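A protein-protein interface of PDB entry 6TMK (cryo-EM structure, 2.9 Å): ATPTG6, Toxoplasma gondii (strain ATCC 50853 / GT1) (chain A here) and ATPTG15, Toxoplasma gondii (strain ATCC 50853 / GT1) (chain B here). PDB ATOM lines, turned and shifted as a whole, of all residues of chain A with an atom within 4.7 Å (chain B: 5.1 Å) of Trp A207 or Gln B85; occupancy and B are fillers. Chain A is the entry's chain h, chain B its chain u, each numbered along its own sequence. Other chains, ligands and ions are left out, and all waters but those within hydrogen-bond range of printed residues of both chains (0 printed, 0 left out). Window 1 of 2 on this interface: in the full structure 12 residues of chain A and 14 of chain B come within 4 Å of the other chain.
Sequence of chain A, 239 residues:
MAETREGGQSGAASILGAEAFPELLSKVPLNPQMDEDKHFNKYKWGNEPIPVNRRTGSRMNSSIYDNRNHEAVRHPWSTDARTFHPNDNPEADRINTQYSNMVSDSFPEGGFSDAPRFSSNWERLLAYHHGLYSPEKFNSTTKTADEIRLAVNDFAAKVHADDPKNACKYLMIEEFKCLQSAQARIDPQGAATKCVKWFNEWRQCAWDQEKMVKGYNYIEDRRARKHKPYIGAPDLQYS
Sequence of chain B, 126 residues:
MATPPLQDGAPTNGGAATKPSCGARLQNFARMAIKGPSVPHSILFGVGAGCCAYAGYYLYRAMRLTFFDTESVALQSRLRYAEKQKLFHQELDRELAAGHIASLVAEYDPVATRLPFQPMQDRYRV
NE2 of His B89 sits at hydrogen-bond distance from O of Arg A203 (3.4 Å).
The side-chain carboxylate of Asp A208 is in salt-bridge range of the side-chain amino group of Lys A211.
The backbone carbonyl oxygen of Lys A211 is in hydrogen-bond range of the backbone NH of Tyr A216, 3.4 Å away.
A ring nitrogen (ND1) of His B89 is in hydrogen-bond range of the backbone carbonyl oxygen (O) of Gln B85 (3.5 Å).
Among the printed residues, merely in contact across the chains: Lys A211 with Tyr B81 (2.9 Å), Glu A210 with Phe B88 (3.4 Å), Trp A207 with Phe B88 (3.6 Å), Trp A207 with Gln B85 (3.6 Å), Ala A206 with Phe B88 (3.6 Å), Tyr A216 with Tyr B81 (3.7 Å), Trp A207 with Tyr B81 (3.8 Å), Trp A207 with His B89 (3.8 Å) and Tyr A216 with Lys B84 (3.998 Å).
Printed residues of chain B within 4 Å of Arg A203: His B89.
Trp A207 touches four residues of chain B.
Of chain A, only Trp A207 (3.6 Å) comes within 4 Å of Gln B85.
Printed residues of chain A within 4 Å of His B89: Arg A203 and Trp A207.
The nearest printed residue of chain A that does not touch Gln B85 is Asp A208 (6.5 Å).
The nearest printed residue of chain A that does not touch Lys B84 is Trp A207 (4.1 Å).
Of the 10 printed residues of chain A, 6 touch a printed residue of chain B.
Hydrophobic or aromatic side chains of chain A within 4 Å of the printed part of chain B: Trp A207 and Tyr A216.
Among the printed residues, 10 pairs touch across the chains.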
ATOM      1  N   ARG A 203     -10.082   1.337 -25.736  1.00  0.00           N
ATOM      2  CA  ARG A 203     -10.463  -0.054 -25.529  1.00  0.00           C
ATOM      3  C   ARG A 203     -11.926  -0.174 -25.122  1.00  0.00           C
ATOM      4  O   ARG A 203     -12.622  -1.103 -25.542  1.00  0.00           O
ATOM      5  CB  ARG A 203      -9.547  -0.660 -24.470  1.00  0.00           C
ATOM      6  CG  ARG A 203      -9.326  -2.129 -24.560  1.00  0.00           C
ATOM      7  CD  ARG A 203      -8.139  -2.542 -23.712  1.00  0.00           C
ATOM      8  NE  ARG A 203      -8.043  -3.989 -23.578  1.00  0.00           N
ATOM      9  CZ  ARG A 203      -8.685  -4.706 -22.665  1.00  0.00           C
ATOM     10  NH1 ARG A 203      -9.479  -4.119 -21.789  1.00  0.00           N
ATOM     11  NH2 ARG A 203      -8.535  -6.019 -22.634  1.00  0.00           N
ATOM     12  N   GLN A 204     -12.398   0.747 -24.287  1.00  0.00           N
ATOM     13  CA  GLN A 204     -13.805   0.752 -23.900  1.00  0.00           C
ATOM     14  C   GLN A 204     -14.705   1.129 -25.072  1.00  0.00           C
ATOM     15  O   GLN A 204     -15.739   0.489 -25.308  1.00  0.00           O
ATOM     16  CB  GLN A 204     -14.006   1.709 -22.735  1.00  0.00           C
ATOM     17  CG  GLN A 204     -13.306   1.285 -21.488  1.00  0.00           C
ATOM     18  CD  GLN A 204     -13.381   2.316 -20.403  1.00  0.00           C
ATOM     19  OE1 GLN A 204     -13.908   3.406 -20.595  1.00  0.00           O
ATOM     20  NE2 GLN A 204     -12.868   1.973 -19.243  1.00  0.00           N
ATOM     21  N   CYS A 205     -14.349   2.195 -25.788  1.00  0.00           N
ATOM     22  CA  CYS A 205     -15.153   2.642 -26.918  1.00  0.00           C
ATOM     23  C   CYS A 205     -15.287   1.557 -27.973  1.00  0.00           C
ATOM     24  O   CYS A 205     -16.323   1.459 -28.638  1.00  0.00           O
ATOM     25  CB  CYS A 205     -14.544   3.907 -27.518  1.00  0.00           C
ATOM     26  SG  CYS A 205     -15.104   4.320 -29.178  1.00  0.00           S
ATOM     27  N   ALA A 206     -14.260   0.726 -28.131  1.00  0.00           N
ATOM     28  CA  ALA A 206     -14.332  -0.353 -29.105  1.00  0.00           C
ATOM     29  C   ALA A 206     -15.475  -1.303 -28.783  1.00  0.00           C
ATOM     30  O   ALA A 206     -16.272  -1.659 -29.659  1.00  0.00           O
ATOM     31  CB  ALA A 206     -13.002  -1.095 -29.144  1.00  0.00           C
ATOM     32  N   TRP A 207     -15.565  -1.737 -27.530  1.00  0.00           N
ATOM     33  CA  TRP A 207     -16.657  -2.611 -27.137  1.00  0.00           C
ATOM     34  C   TRP A 207     -17.999  -1.898 -27.192  1.00  0.00           C
ATOM     35  O   TRP A 207     -19.007  -2.503 -27.566  1.00  0.00           O
ATOM     36  CB  TRP A 207     -16.395  -3.157 -25.739  1.00  0.00           C
ATOM     37  CG  TRP A 207     -17.596  -3.733 -25.083  1.00  0.00           C
ATOM     38  CD1 TRP A 207     -18.234  -3.246 -23.990  1.00  0.00           C
ATOM     39  CD2 TRP A 207     -18.322  -4.894 -25.483  1.00  0.00           C
ATOM     40  NE1 TRP A 207     -19.306  -4.028 -23.679  1.00  0.00           N
ATOM     41  CE2 TRP A 207     -19.383  -5.050 -24.583  1.00  0.00           C
ATOM     42  CE3 TRP A 207     -18.178  -5.816 -26.514  1.00  0.00           C
ATOM     43  CZ2 TRP A 207     -20.287  -6.088 -24.679  1.00  0.00           C
ATOM     44  CZ3 TRP A 207     -19.075  -6.844 -26.601  1.00  0.00           C
ATOM     45  CH2 TRP A 207     -20.115  -6.972 -25.694  1.00  0.00           C
ATOM     46  N   ASP A 208     -18.048  -0.627 -26.795  1.00  0.00           N
ATOM     47  CA  ASP A 208     -19.316   0.088 -26.858  1.00  0.00           C
ATOM     48  C   ASP A 208     -19.832   0.197 -28.289  1.00  0.00           C
ATOM     49  O   ASP A 208     -21.036   0.013 -28.543  1.00  0.00           O
ATOM     50  CB  ASP A 208     -19.140   1.473 -26.243  1.00  0.00           C
ATOM     51  CG  ASP A 208     -18.810   1.418 -24.768  1.00  0.00           C
ATOM     52  OD1 ASP A 208     -19.080   0.381 -24.134  1.00  0.00           O
ATOM     53  OD2 ASP A 208     -18.269   2.414 -24.246  1.00  0.00           O
ATOM     54  N   GLN A 209     -18.917   0.288 -29.250  1.00  0.00           N
ATOM     55  CA  GLN A 209     -19.317   0.326 -30.645  1.00  0.00           C
ATOM     56  C   GLN A 209     -19.706  -1.055 -31.134  1.00  0.00           C
ATOM     57  O   GLN A 209     -20.668  -1.191 -31.893  1.00  0.00           O
ATOM     58  CB  GLN A 209     -18.189   0.914 -31.489  1.00  0.00           C
ATOM     59  CG  GLN A 209     -18.611   1.434 -32.844  1.00  0.00           C
ATOM     60  CD  GLN A 209     -17.458   1.968 -33.674  1.00  0.00           C
ATOM     61  OE1 GLN A 209     -17.673   2.532 -34.746  1.00  0.00           O
ATOM     62  NE2 GLN A 209     -16.235   1.812 -33.181  1.00  0.00           N
ATOM     63  N   GLU A 210     -18.952  -2.085 -30.755  1.00  0.00           N
ATOM     64  CA  GLU A 210     -19.314  -3.418 -31.208  1.00  0.00           C
ATOM     65  C   GLU A 210     -20.690  -3.795 -30.687  1.00  0.00           C
ATOM     66  O   GLU A 210     -21.481  -4.413 -31.403  1.00  0.00           O
ATOM     67  CB  GLU A 210     -18.277  -4.434 -30.752  1.00  0.00           C
ATOM     68  CG  GLU A 210     -18.380  -5.760 -31.460  1.00  0.00           C
ATOM     69  CD  GLU A 210     -17.761  -5.732 -32.842  1.00  0.00           C
ATOM     70  OE1 GLU A 210     -17.464  -4.626 -33.337  1.00  0.00           O
ATOM     71  OE2 GLU A 210     -17.576  -6.816 -33.436  1.00  0.00           O
ATOM     72  N   LYS A 211     -20.983  -3.459 -29.430  1.00  0.00           N
ATOM     73  CA  LYS A 211     -22.269  -3.820 -28.856  1.00  0.00           C
ATOM     74  C   LYS A 211     -23.399  -2.964 -29.401  1.00  0.00           C
ATOM     75  O   LYS A 211     -24.560  -3.370 -29.313  1.00  0.00           O
ATOM     76  CB  LYS A 211     -22.244  -3.714 -27.339  1.00  0.00           C
ATOM     77  CG  LYS A 211     -22.142  -2.324 -26.812  1.00  0.00           C
ATOM     78  CD  LYS A 211     -22.220  -2.323 -25.328  1.00  0.00           C
ATOM     79  CE  LYS A 211     -22.228  -0.932 -24.769  1.00  0.00           C
ATOM     80  NZ  LYS A 211     -21.376  -0.786 -23.567  1.00  0.00           N
ATOM     81  N   TYR A 216     -26.405  -6.095 -28.566  1.00  0.00           N
ATOM     82  CA  TYR A 216     -26.179  -6.891 -27.371  1.00  0.00           C
ATOM     83  C   TYR A 216     -26.797  -6.145 -26.204  1.00  0.00           C
ATOM     84  O   TYR A 216     -26.473  -4.979 -25.966  1.00  0.00           O
ATOM     85  CB  TYR A 216     -24.690  -7.134 -27.118  1.00  0.00           C
ATOM     86  CG  TYR A 216     -24.002  -8.052 -28.091  1.00  0.00           C
ATOM     87  CD1 TYR A 216     -24.685  -9.076 -28.717  1.00  0.00           C
ATOM     88  CD2 TYR A 216     -22.657  -7.908 -28.363  1.00  0.00           C
ATOM     89  CE1 TYR A 216     -24.051  -9.912 -29.598  1.00  0.00           C
ATOM     90  CE2 TYR A 216     -22.018  -8.739 -29.237  1.00  0.00           C
ATOM     91  CZ  TYR A 216     -22.715  -9.742 -29.851  1.00  0.00           C
ATOM     92  OH  TYR A 216     -22.066 -10.572 -30.728  1.00  0.00           O
ATOM     93  N   TYR B  81     -23.752 -11.476 -21.096  1.00  0.00           N
ATOM     94  CA  TYR B  81     -23.230 -10.223 -21.626  1.00  0.00           C
ATOM     95  C   TYR B  81     -21.757 -10.052 -21.275  1.00  0.00           C
ATOM     96  O   TYR B  81     -20.941  -9.660 -22.122  1.00  0.00           O
ATOM     97  CB  TYR B  81     -24.072  -9.078 -21.072  1.00  0.00           C
ATOM     98  CG  TYR B  81     -23.770  -7.702 -21.593  1.00  0.00           C
ATOM     99  CD1 TYR B  81     -24.489  -7.181 -22.644  1.00  0.00           C
ATOM    100  CD2 TYR B  81     -22.798  -6.911 -21.017  1.00  0.00           C
ATOM    101  CE1 TYR B  81     -24.241  -5.932 -23.114  1.00  0.00           C
ATOM    102  CE2 TYR B  81     -22.542  -5.664 -21.486  1.00  0.00           C
ATOM    103  CZ  TYR B  81     -23.267  -5.174 -22.534  1.00  0.00           C
ATOM    104  OH  TYR B  81     -23.012  -3.914 -23.003  1.00  0.00           O
ATOM    105  N   ALA B  82     -21.397 -10.354 -20.026  1.00  0.00           N
ATOM    106  CA  ALA B  82     -20.013 -10.234 -19.598  1.00  0.00           C
ATOM    107  C   ALA B  82     -19.110 -11.182 -20.370  1.00  0.00           C
ATOM    108  O   ALA B  82     -17.965 -10.844 -20.679  1.00  0.00           O
ATOM    109  CB  ALA B  82     -19.919 -10.506 -18.103  1.00  0.00           C
ATOM    110  N   GLU B  83     -19.598 -12.383 -20.666  1.00  0.00           N
ATOM    111  CA  GLU B  83     -18.809 -13.332 -21.441  1.00  0.00           C
ATOM    112  C   GLU B  83     -18.516 -12.788 -22.832  1.00  0.00           C
ATOM    113  O   GLU B  83     -17.378 -12.853 -23.318  1.00  0.00           O
ATOM    114  CB  GLU B  83     -19.546 -14.659 -21.535  1.00  0.00           C
ATOM    115  CG  GLU B  83     -18.655 -15.825 -21.847  1.00  0.00           C
ATOM    116  CD  GLU B  83     -19.431 -17.031 -22.307  1.00  0.00           C
ATOM    117  OE1 GLU B  83     -20.659 -17.064 -22.089  1.00  0.00           O
ATOM    118  OE2 GLU B  83     -18.818 -17.945 -22.892  1.00  0.00           O
ATOM    119  N   LYS B  84     -19.548 -12.269 -23.499  1.00  0.00           N
ATOM    120  CA  LYS B  84     -19.345 -11.661 -24.810  1.00  0.00           C
ATOM    121  C   LYS B  84     -18.311 -10.544 -24.743  1.00  0.00           C
ATOM    122  O   LYS B  84     -17.411 -10.456 -25.588  1.00  0.00           O
ATOM    123  CB  LYS B  84     -20.674 -11.137 -25.335  1.00  0.00           C
ATOM    124  CG  LYS B  84     -21.613 -12.209 -25.750  1.00  0.00           C
ATOM    125  CD  LYS B  84     -22.937 -11.655 -26.177  1.00  0.00           C
ATOM    126  CE  LYS B  84     -23.921 -12.766 -26.463  1.00  0.00           C
ATOM    127  NZ  LYS B  84     -24.775 -13.076 -25.286  1.00  0.00           N
ATOM    128  N   GLN B  85     -18.429  -9.684 -23.734  1.00  0.00           N
ATOM    129  CA  GLN B  85     -17.500  -8.574 -23.563  1.00  0.00           C
ATOM    130  C   GLN B  85     -16.072  -9.074 -23.376  1.00  0.00           C
ATOM    131  O   GLN B  85     -15.124  -8.557 -23.984  1.00  0.00           O
ATOM    132  CB  GLN B  85     -17.959  -7.742 -22.375  1.00  0.00           C
ATOM    133  CG  GLN B  85     -17.090  -6.605 -22.000  1.00  0.00           C
ATOM    134  CD  GLN B  85     -17.727  -5.749 -20.944  1.00  0.00           C
ATOM    135  OE1 GLN B  85     -18.803  -6.061 -20.444  1.00  0.00           O
ATOM    136  NE2 GLN B  85     -17.072  -4.669 -20.594  1.00  0.00           N
ATOM    137  N   LYS B  86     -15.909 -10.083 -22.524  1.00  0.00           N
ATOM    138  CA  LYS B  86     -14.604 -10.666 -22.259  1.00  0.00           C
ATOM    139  C   LYS B  86     -13.963 -11.174 -23.539  1.00  0.00           C
ATOM    140  O   LYS B  86     -12.792 -10.894 -23.817  1.00  0.00           O
ATOM    141  CB  LYS B  86     -14.766 -11.805 -21.262  1.00  0.00           C
ATOM    142  CG  LYS B  86     -13.495 -12.343 -20.683  1.00  0.00           C
ATOM    143  CD  LYS B  86     -13.673 -13.772 -20.245  1.00  0.00           C
ATOM    144  CE  LYS B  86     -14.502 -13.871 -18.990  1.00  0.00           C
ATOM    145  NZ  LYS B  86     -15.184 -15.185 -18.920  1.00  0.00           N
ATOM    146  N   LEU B  87     -14.716 -11.944 -24.321  1.00  0.00           N
ATOM    147  CA  LEU B  87     -14.139 -12.540 -25.516  1.00  0.00           C
ATOM    148  C   LEU B  87     -13.813 -11.480 -26.558  1.00  0.00           C
ATOM    149  O   LEU B  87     -12.800 -11.585 -27.261  1.00  0.00           O
ATOM    150  CB  LEU B  87     -15.088 -13.591 -26.071  1.00  0.00           C
ATOM    151  CG  LEU B  87     -15.430 -14.728 -25.116  1.00  0.00           C
ATOM    152  CD1 LEU B  87     -16.208 -15.775 -25.846  1.00  0.00           C
ATOM    153  CD2 LEU B  87     -14.204 -15.332 -24.481  1.00  0.00           C
ATOM    154  N   PHE B  88     -14.639 -10.439 -26.653  1.00  0.00           N
ATOM    155  CA  PHE B  88     -14.318  -9.331 -27.540  1.00  0.00           C
ATOM    156  C   PHE B  88     -12.980  -8.703 -27.173  1.00  0.00           C
ATOM    157  O   PHE B  88     -12.106  -8.522 -28.031  1.00  0.00           O
ATOM    158  CB  PHE B  88     -15.421  -8.278 -27.484  1.00  0.00           C
ATOM    159  CG  PHE B  88     -15.129  -7.073 -28.308  1.00  0.00           C
ATOM    160  CD1 PHE B  88     -15.460  -7.036 -29.638  1.00  0.00           C
ATOM    161  CD2 PHE B  88     -14.495  -5.983 -27.755  1.00  0.00           C
ATOM    162  CE1 PHE B  88     -15.176  -5.936 -30.395  1.00  0.00           C
ATOM    163  CE2 PHE B  88     -14.210  -4.890 -28.509  1.00  0.00           C
ATOM    164  CZ  PHE B  88     -14.545  -4.865 -29.830  1.00  0.00           C
ATOM    165  N   HIS B  89     -12.816  -8.338 -25.901  1.00  0.00           N
ATOM    166  CA  HIS B  89     -11.578  -7.698 -25.472  1.00  0.00           C
ATOM    167  C   HIS B  89     -10.376  -8.604 -25.694  1.00  0.00           C
ATOM    168  O   HIS B  89      -9.304  -8.146 -26.110  1.00  0.00           O
ATOM    169  CB  HIS B  89     -11.694  -7.306 -24.004  1.00  0.00           C
ATOM    170  CG  HIS B  89     -12.414  -6.017 -23.778  1.00  0.00           C
ATOM    171  ND1 HIS B  89     -13.312  -5.838 -22.751  1.00  0.00           N
ATOM    172  CD2 HIS B  89     -12.341  -4.832 -24.426  1.00  0.00           C
ATOM    173  CE1 HIS B  89     -13.782  -4.606 -22.791  1.00  0.00           C
ATOM    174  NE2 HIS B  89     -13.208  -3.974 -23.797  1.00  0.00           N
ATOM    175  N   GLN B  90     -10.544  -9.895 -25.427  1.00  0.00           N
ATOM    176  CA  GLN B  90      -9.477 -10.858 -25.658  1.00  0.00           C
ATOM    177  C   GLN B  90      -9.032 -10.849 -27.116  1.00  0.00           C
ATOM    178  O   GLN B  90      -7.839 -10.705 -27.420  1.00  0.00           O
ATOM    179  CB  GLN B  90      -9.973 -12.235 -25.238  1.00  0.00           C
ATOM    180  CG  GLN B  90      -8.924 -13.222 -24.875  1.00  0.00           C
ATOM    181  CD  GLN B  90      -9.499 -14.396 -24.126  1.00  0.00           C
ATOM    182  OE1 GLN B  90     -10.168 -14.228 -23.108  1.00  0.00           O
ATOM    183  NE2 GLN B  90      -9.273 -15.594 -24.644  1.00  0.00           N
